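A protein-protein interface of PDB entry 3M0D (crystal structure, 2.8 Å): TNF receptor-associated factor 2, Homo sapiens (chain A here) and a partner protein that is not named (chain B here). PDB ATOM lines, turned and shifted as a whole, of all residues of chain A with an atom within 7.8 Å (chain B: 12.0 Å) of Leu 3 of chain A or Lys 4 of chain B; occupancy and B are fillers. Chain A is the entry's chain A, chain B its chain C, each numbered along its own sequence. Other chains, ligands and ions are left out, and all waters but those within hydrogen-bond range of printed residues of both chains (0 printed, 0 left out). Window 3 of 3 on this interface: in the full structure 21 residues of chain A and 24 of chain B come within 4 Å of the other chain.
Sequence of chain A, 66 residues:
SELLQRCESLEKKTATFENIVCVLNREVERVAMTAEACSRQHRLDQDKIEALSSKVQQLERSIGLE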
ATOM      1  N   GLU A   2       1.083  12.843 -17.169  1.00  0.00           N
ATOM      2  CA  GLU A   2       1.822  12.926 -15.918  1.00  0.00           C
ATOM      3  C   GLU A   2       0.943  13.438 -14.791  1.00  0.00           C
ATOM      4  O   GLU A   2       0.321  12.652 -14.081  1.00  0.00           O
ATOM      5  CB  GLU A   2       3.074  13.807 -16.059  1.00  0.00           C
ATOM      6  CG  GLU A   2       4.024  13.735 -14.861  1.00  0.00           C
ATOM      7  CD  GLU A   2       4.479  12.312 -14.562  1.00  0.00           C
ATOM      8  OE1 GLU A   2       5.003  11.659 -15.491  1.00  0.00           O
ATOM      9  OE2 GLU A   2       4.306  11.847 -13.408  1.00  0.00           O
ATOM     10  N   LEU A   3       0.888  14.757 -14.626  1.00  0.00           N
ATOM     11  CA  LEU A   3       0.236  15.356 -13.458  1.00  0.00           C
ATOM     12  C   LEU A   3      -1.265  15.167 -13.429  1.00  0.00           C
ATOM     13  O   LEU A   3      -1.872  15.136 -12.362  1.00  0.00           O
ATOM     14  CB  LEU A   3       0.534  16.843 -13.360  1.00  0.00           C
ATOM     15  CG  LEU A   3       0.120  17.399 -12.002  1.00  0.00           C
ATOM     16  CD1 LEU A   3       1.032  16.810 -10.927  1.00  0.00           C
ATOM     17  CD2 LEU A   3       0.177  18.921 -11.991  1.00  0.00           C
ATOM     18  N   LEU A   4      -1.862  15.055 -14.605  1.00  0.00           N
ATOM     19  CA  LEU A   4      -3.292  14.859 -14.710  1.00  0.00           C
ATOM     20  C   LEU A   4      -3.668  13.484 -14.183  1.00  0.00           C
ATOM     21  O   LEU A   4      -4.557  13.344 -13.339  1.00  0.00           O
ATOM     22  CB  LEU A   4      -3.709  14.984 -16.163  1.00  0.00           C
ATOM     23  CG  LEU A   4      -5.109  15.523 -16.428  1.00  0.00           C
ATOM     24  CD1 LEU A   4      -5.235  15.944 -17.890  1.00  0.00           C
ATOM     25  CD2 LEU A   4      -6.170  14.495 -16.047  1.00  0.00           C
ATOM     26  N   GLN A   5      -2.983  12.462 -14.680  1.00  0.00           N
ATOM     27  CA  GLN A   5      -3.277  11.100 -14.256  1.00  0.00           C
ATOM     28  C   GLN A   5      -2.858  10.827 -12.790  1.00  0.00           C
ATOM     29  O   GLN A   5      -3.460   9.988 -12.109  1.00  0.00           O
ATOM     30  CB  GLN A   5      -2.696  10.072 -15.251  1.00  0.00           C
ATOM     31  CG  GLN A   5      -1.206  10.205 -15.552  1.00  0.00           C
ATOM     32  CD  GLN A   5      -0.315   9.552 -14.494  1.00  0.00           C
ATOM     33  OE1 GLN A   5       0.822   9.988 -14.263  1.00  0.00           O
ATOM     34  NE2 GLN A   5      -0.825   8.498 -13.851  1.00  0.00           N
ATOM     35  N   ARG A   6      -1.841  11.548 -12.314  1.00  0.00           N
ATOM     36  CA  ARG A   6      -1.419  11.443 -10.921  1.00  0.00           C
ATOM     37  C   ARG A   6      -2.538  11.922 -10.030  1.00  0.00           C
ATOM     38  O   ARG A   6      -2.913  11.258  -9.084  1.00  0.00           O
ATOM     39  CB  ARG A   6      -0.174  12.288 -10.646  1.00  0.00           C
ATOM     40  CG  ARG A   6       1.111  11.492 -10.651  1.00  0.00           C
ATOM     41  CD  ARG A   6       2.293  12.335 -10.238  1.00  0.00           C
ATOM     42  NE  ARG A   6       3.528  11.578 -10.377  1.00  0.00           N
ATOM     43  CZ  ARG A   6       4.040  10.816  -9.418  1.00  0.00           C
ATOM     44  NH1 ARG A   6       3.425  10.722  -8.249  1.00  0.00           N
ATOM     45  NH2 ARG A   6       5.169  10.153  -9.623  1.00  0.00           N
ATOM     46  N   CYS A   7      -3.069  13.091 -10.347  1.00  0.00           N
ATOM     47  CA  CYS A   7      -4.168  13.663  -9.597  1.00  0.00           C
ATOM     48  C   CYS A   7      -5.457  12.835  -9.694  1.00  0.00           C
ATOM     49  O   CYS A   7      -6.149  12.652  -8.698  1.00  0.00           O
ATOM     50  CB  CYS A   7      -4.394  15.107 -10.040  1.00  0.00           C
ATOM     51  SG  CYS A   7      -5.997  15.795  -9.633  1.00  0.00           S
ATOM     52  N   GLU A   8      -5.782  12.329 -10.878  1.00  0.00           N
ATOM     53  CA  GLU A   8      -6.958  11.482 -11.027  1.00  0.00           C
ATOM     54  C   GLU A   8      -6.852  10.203 -10.162  1.00  0.00           C
ATOM     55  O   GLU A   8      -7.817   9.782  -9.508  1.00  0.00           O
ATOM     56  CB  GLU A   8      -7.163  11.133 -12.502  1.00  0.00           C
ATOM     57  N   SER A   9      -5.662   9.607 -10.161  1.00  0.00           N
ATOM     58  CA  SER A   9      -5.357   8.393  -9.398  1.00  0.00           C
ATOM     59  C   SER A   9      -5.462   8.590  -7.894  1.00  0.00           C
ATOM     60  O   SER A   9      -5.955   7.728  -7.161  1.00  0.00           O
ATOM     61  CB  SER A   9      -3.931   7.939  -9.716  1.00  0.00           C
ATOM     62  OG  SER A   9      -3.282   7.424  -8.567  1.00  0.00           O
ATOM     63  N   PHE B   2       9.417  20.936 -12.425  1.00  0.00           N
ATOM     64  CA  PHE B   2       8.145  20.291 -12.124  1.00  0.00           C
ATOM     65  C   PHE B   2       8.038  19.891 -10.642  1.00  0.00           C
ATOM     66  O   PHE B   2       8.461  18.798 -10.248  1.00  0.00           O
ATOM     67  CB  PHE B   2       7.967  19.064 -13.015  1.00  0.00           C
ATOM     68  CG  PHE B   2       6.535  18.645 -13.197  1.00  0.00           C
ATOM     69  CD1 PHE B   2       6.224  17.466 -13.873  1.00  0.00           C
ATOM     70  CD2 PHE B   2       5.499  19.428 -12.709  1.00  0.00           C
ATOM     71  CE1 PHE B   2       4.901  17.063 -14.049  1.00  0.00           C
ATOM     72  CE2 PHE B   2       4.181  19.037 -12.885  1.00  0.00           C
ATOM     73  CZ  PHE B   2       3.883  17.851 -13.557  1.00  0.00           C
ATOM     74  N   MET B   3       7.462  20.772  -9.825  1.00  0.00           N
ATOM     75  CA  MET B   3       7.370  20.521  -8.389  1.00  0.00           C
ATOM     76  C   MET B   3       5.975  20.144  -7.900  1.00  0.00           C
ATOM     77  O   MET B   3       5.831  19.606  -6.808  1.00  0.00           O
ATOM     78  CB  MET B   3       7.930  21.690  -7.570  1.00  0.00           C
ATOM     79  CG  MET B   3       7.055  22.930  -7.533  1.00  0.00           C
ATOM     80  SD  MET B   3       7.964  24.341  -6.854  1.00  0.00           S
ATOM     81  CE  MET B   3       9.439  24.370  -7.882  1.00  0.00           C
ATOM     82  N   LYS B   4       4.943  20.407  -8.688  1.00  0.00           N
ATOM     83  CA  LYS B   4       3.630  19.900  -8.309  1.00  0.00           C
ATOM     84  C   LYS B   4       3.512  18.384  -8.458  1.00  0.00           C
ATOM     85  O   LYS B   4       2.733  17.766  -7.745  1.00  0.00           O
ATOM     86  CB  LYS B   4       2.486  20.622  -9.025  1.00  0.00           C
ATOM     87  CG  LYS B   4       2.026  21.872  -8.295  1.00  0.00           C
ATOM     88  CD  LYS B   4       0.566  22.168  -8.581  1.00  0.00           C
ATOM     89  CE  LYS B   4       0.034  23.277  -7.682  1.00  0.00           C
ATOM     90  NZ  LYS B   4       0.139  22.939  -6.230  1.00  0.00           N
ATOM     91  N   GLU B   5       4.282  17.771  -9.354  1.00  0.00           N
ATOM     92  CA  GLU B   5       4.259  16.310  -9.428  1.00  0.00           C
ATOM     93  C   GLU B   5       5.000  15.705  -8.231  1.00  0.00           C
ATOM     94  O   GLU B   5       4.771  14.545  -7.857  1.00  0.00           O
ATOM     95  CB  GLU B   5       4.842  15.796 -10.743  1.00  0.00           C
ATOM     96  CG  GLU B   5       6.357  15.792 -10.803  1.00  0.00           C
ATOM     97  CD  GLU B   5       6.879  14.962 -11.962  1.00  0.00           C
ATOM     98  OE1 GLU B   5       6.122  14.087 -12.448  1.00  0.00           O
ATOM     99  OE2 GLU B   5       8.036  15.193 -12.392  1.00  0.00           O
ATOM    100  N   LYS B   6       5.881  16.509  -7.637  1.00  0.00           N
ATOM    101  CA  LYS B   6       6.654  16.102  -6.475  1.00  0.00           C
ATOM    102  C   LYS B   6       5.790  16.217  -5.207  1.00  0.00           C
ATOM    103  O   LYS B   6       5.922  15.443  -4.262  1.00  0.00           O
ATOM    104  CB  LYS B   6       7.920  16.959  -6.362  1.00  0.00           C
ATOM    105  CG  LYS B   6       9.084  16.282  -5.641  1.00  0.00           C
ATOM    106  CD  LYS B   6      10.298  17.214  -5.447  1.00  0.00           C
ATOM    107  CE  LYS B   6      11.355  16.543  -4.551  1.00  0.00           C
ATOM    108  NZ  LYS B   6      12.555  17.387  -4.259  1.00  0.00           N
ATOM    109  N   LEU B   7       4.904  17.201  -5.194  1.00  0.00           N
ATOM    110  CA  LEU B   7       3.926  17.322  -4.130  1.00  0.00           C
ATOM    111  C   LEU B   7       3.075  16.070  -4.147  1.00  0.00           C
ATOM    112  O   LEU B   7       3.056  15.304  -3.179  1.00  0.00           O
ATOM    113  CB  LEU B   7       3.047  18.557  -4.358  1.00  0.00           C
ATOM    114  CG  LEU B   7       1.801  18.793  -3.494  1.00  0.00           C
ATOM    115  CD1 LEU B   7       2.145  19.062  -2.028  1.00  0.00           C
ATOM    116  CD2 LEU B   7       0.977  19.941  -4.059  1.00  0.00           C
ATOM    117  N   LEU B   8       2.372  15.870  -5.259  1.00  0.00           N
ATOM    118  CA  LEU B   8       1.521  14.703  -5.450  1.00  0.00           C
ATOM    119  C   LEU B   8       2.169  13.377  -5.047  1.00  0.00           C
ATOM    120  O   LEU B   8       1.496  12.496  -4.492  1.00  0.00           O
ATOM    121  CB  LEU B   8       1.060  14.633  -6.897  1.00  0.00           C
ATOM    122  CG  LEU B   8      -0.360  15.146  -7.100  1.00  0.00           C
ATOM    123  CD1 LEU B   8      -0.570  16.381  -6.276  1.00  0.00           C
ATOM    124  CD2 LEU B   8      -0.641  15.392  -8.571  1.00  0.00           C
ATOM    125  N   ALA B   9       3.460  13.225  -5.335  1.00  0.00           N
ATOM    126  CA  ALA B   9       4.199  12.054  -4.883  1.00  0.00           C
ATOM    127  C   ALA B   9       4.190  12.011  -3.363  1.00  0.00           C
ATOM    128  O   ALA B   9       3.831  11.005  -2.762  1.00  0.00           O
ATOM    129  CB  ALA B   9       5.613  12.087  -5.399  1.00  0.00           C
ATOM    130  N   GLU B  10       4.585  13.117  -2.750  1.00  0.00           N
ATOM    131  CA  GLU B  10       4.561  13.263  -1.307  1.00  0.00           C
ATOM    132  C   GLU B  10       3.232  12.773  -0.717  1.00  0.00           C
ATOM    133  O   GLU B  10       3.210  11.970   0.222  1.00  0.00           O
ATOM    134  CB  GLU B  10       4.779  14.734  -0.941  1.00  0.00           C
ATOM    135  CG  GLU B  10       5.092  14.991   0.518  1.00  0.00           C
ATOM    136  CD  GLU B  10       6.574  14.855   0.828  1.00  0.00           C
ATOM    137  OE1 GLU B  10       6.916  14.392   1.948  1.00  0.00           O
ATOM    138  OE2 GLU B  10       7.394  15.218  -0.050  1.00  0.00           O
ATOM    139  N   LEU B  11       2.130  13.273  -1.264  1.00  0.00           N
ATOM    140  CA  LEU B  11       0.808  12.866  -0.811  1.00  0.00           C
ATOM    141  C   LEU B  11       0.536  11.364  -0.968  1.00  0.00           C
ATOM    142  O   LEU B  11       0.084  10.720  -0.019  1.00  0.00           O
ATOM    143  CB  LEU B  11      -0.275  13.679  -1.516  1.00  0.00           C
ATOM    144  CG  LEU B  11      -0.109  15.184  -1.305  1.00  0.00           C
ATOM    145  CD1 LEU B  11      -1.411  15.949  -1.569  1.00  0.00           C
ATOM    146  CD2 LEU B  11       0.415  15.490   0.090  1.00  0.00           C
ATOM    147  N   GLU B  12       0.805  10.811  -2.151  1.00  0.00           N
ATOM    148  CA  GLU B  12       0.564   9.393  -2.395  1.00  0.00           C
ATOM    149  C   GLU B  12       1.202   8.525  -1.305  1.00  0.00           C
ATOM    150  O   GLU B  12       0.573   7.581  -0.809  1.00  0.00           O
ATOM    151  CB  GLU B  12       1.055   8.978  -3.794  1.00  0.00           C
ATOM    152  CG  GLU B  12       0.167   9.508  -4.937  1.00  0.00           C
ATOM    153  CD  GLU B  12       0.787   9.378  -6.338  1.00  0.00           C
ATOM    154  OE1 GLU B  12       0.017   9.395  -7.332  1.00  0.00           O
ATOM    155  OE2 GLU B  12       2.033   9.278  -6.453  1.00  0.00           O
ATOM    156  N   GLY B  13       2.441   8.849  -0.933  1.00  0.00           N
ATOM    157  CA  GLY B  13       3.164   8.088   0.069  1.00  0.00           C
ATOM    158  C   GLY B  13       2.600   8.185   1.485  1.00  0.00           C
ATOM    159  O   GLY B  13       2.458   7.178   2.207  1.00  0.00           O
ATOM    160  N   LYS B  14       2.304   9.408   1.899  1.00  0.00           N
ATOM    161  CA  LYS B  14       1.649   9.611   3.163  1.00  0.00           C
ATOM    162  C   LYS B  14       0.343   8.841   3.194  1.00  0.00           C
ATOM    163  O   LYS B  14       0.069   8.092   4.139  1.00  0.00           O
ATOM    164  CB  LYS B  14       1.400  11.100   3.395  1.00  0.00           C
ATOM    165  CG  LYS B  14       2.546  11.825   4.063  1.00  0.00           C
ATOM    166  CD  LYS B  14       2.304  13.317   4.019  1.00  0.00           C
ATOM    167  CE  LYS B  14       3.615  14.087   3.972  1.00  0.00           C
ATOM    168  NZ  LYS B  14       3.348  15.533   3.763  1.00  0.00           N
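O of Glu 2 of chain A sits close to OE1 of Gln 5 of chain A (2.7 Å).
The side-chain carboxylate of Glu 2 of chain A lies within salt-bridge range of the guanidinium group of Arg 6 of chain A (3.1 Å).
Of the 13 printed residues of chain B, 6 touch a printed residue of chain A.
Hydrophobic or aromatic side chains of chain B that line the printed part of chain A: Phe 2, Leu 8 and Ala 9.
Hydrophobic or aromatic side chains of chain A within 4 Å of the printed part of chain B: Leu 3.
Among the printed residues, Asp or Glu carboxylates within 4 Å of a Lys or Arg side-chain nitrogen of the other chain: Arg 6 of chain A with Glu 12 of chain B (2.7 Å).
The side-chain carboxylate (OE2) of Glu 12 of chain B is in salt-bridge range of the guanidinium group (NH1) of Arg 6 of chain A (2.7 Å).
OE1 of Glu 5 of chain B lies close to OE2 of Glu 2 of chain A.
Phe 2 of chain B touches Glu 2 of chain A (CE1 to CG, 3.5 Å).
Leu 3 of chain A touches Phe 2 of chain B.
Leu 3 of chain A touches Lys 4 of chain B (CD1 to O, 3.7 Å).
Leu 3 of chain A touches Glu 5 of chain B (CD1 to CA, 3.6 Å).
Leu 3 of chain A touches Leu 8 of chain B (CD1 to CD2, 3.2 Å).
Arg 6 of chain A touches Leu 8 of chain B (CB to CD2, 3.8 Å).
NH1 of Arg 6 of chain A touches CA of Ala 9 of chain B, at 3.7 Å.
Leu 8 of chain B touches Cys 7 of chain A (CD2 to N, 3.8 Å).
Lys 4 of chain B touches just one residue of chain A: Leu 3.
Printed residues of chain B within 4 Å of Glu 2 of chain A: Phe 2 and Glu 5.
Leu 4 of chain A touches none of the printed residues of chain B.
Arg 6 of chain A touches just these residues of chain B: Leu 8 (3.8 Å), Ala 9 (3.7 Å) and Glu 12 (2.7 Å).
Of chain B, only Leu 8 (3.8 Å) comes within 4 Å of Cys 7 of chain A.
Of the printed residues of chain A, Ala 9 of chain B touches Arg 6.
Of the printed residues of chain A, Glu 12 of chain B touches Arg 6.
Of the printed residues of chain A, Glu 5 of chain B touches Glu 2 and Leu 3.
Of the printed residues of chain A, Phe 2 of chain B touches Glu 2 (3.5 Å) and Leu 3 (3.5 Å).
The nearest residue of chain B that does not touch Leu 3 of chain A is Lys 6 of chain B (5.9 Å).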
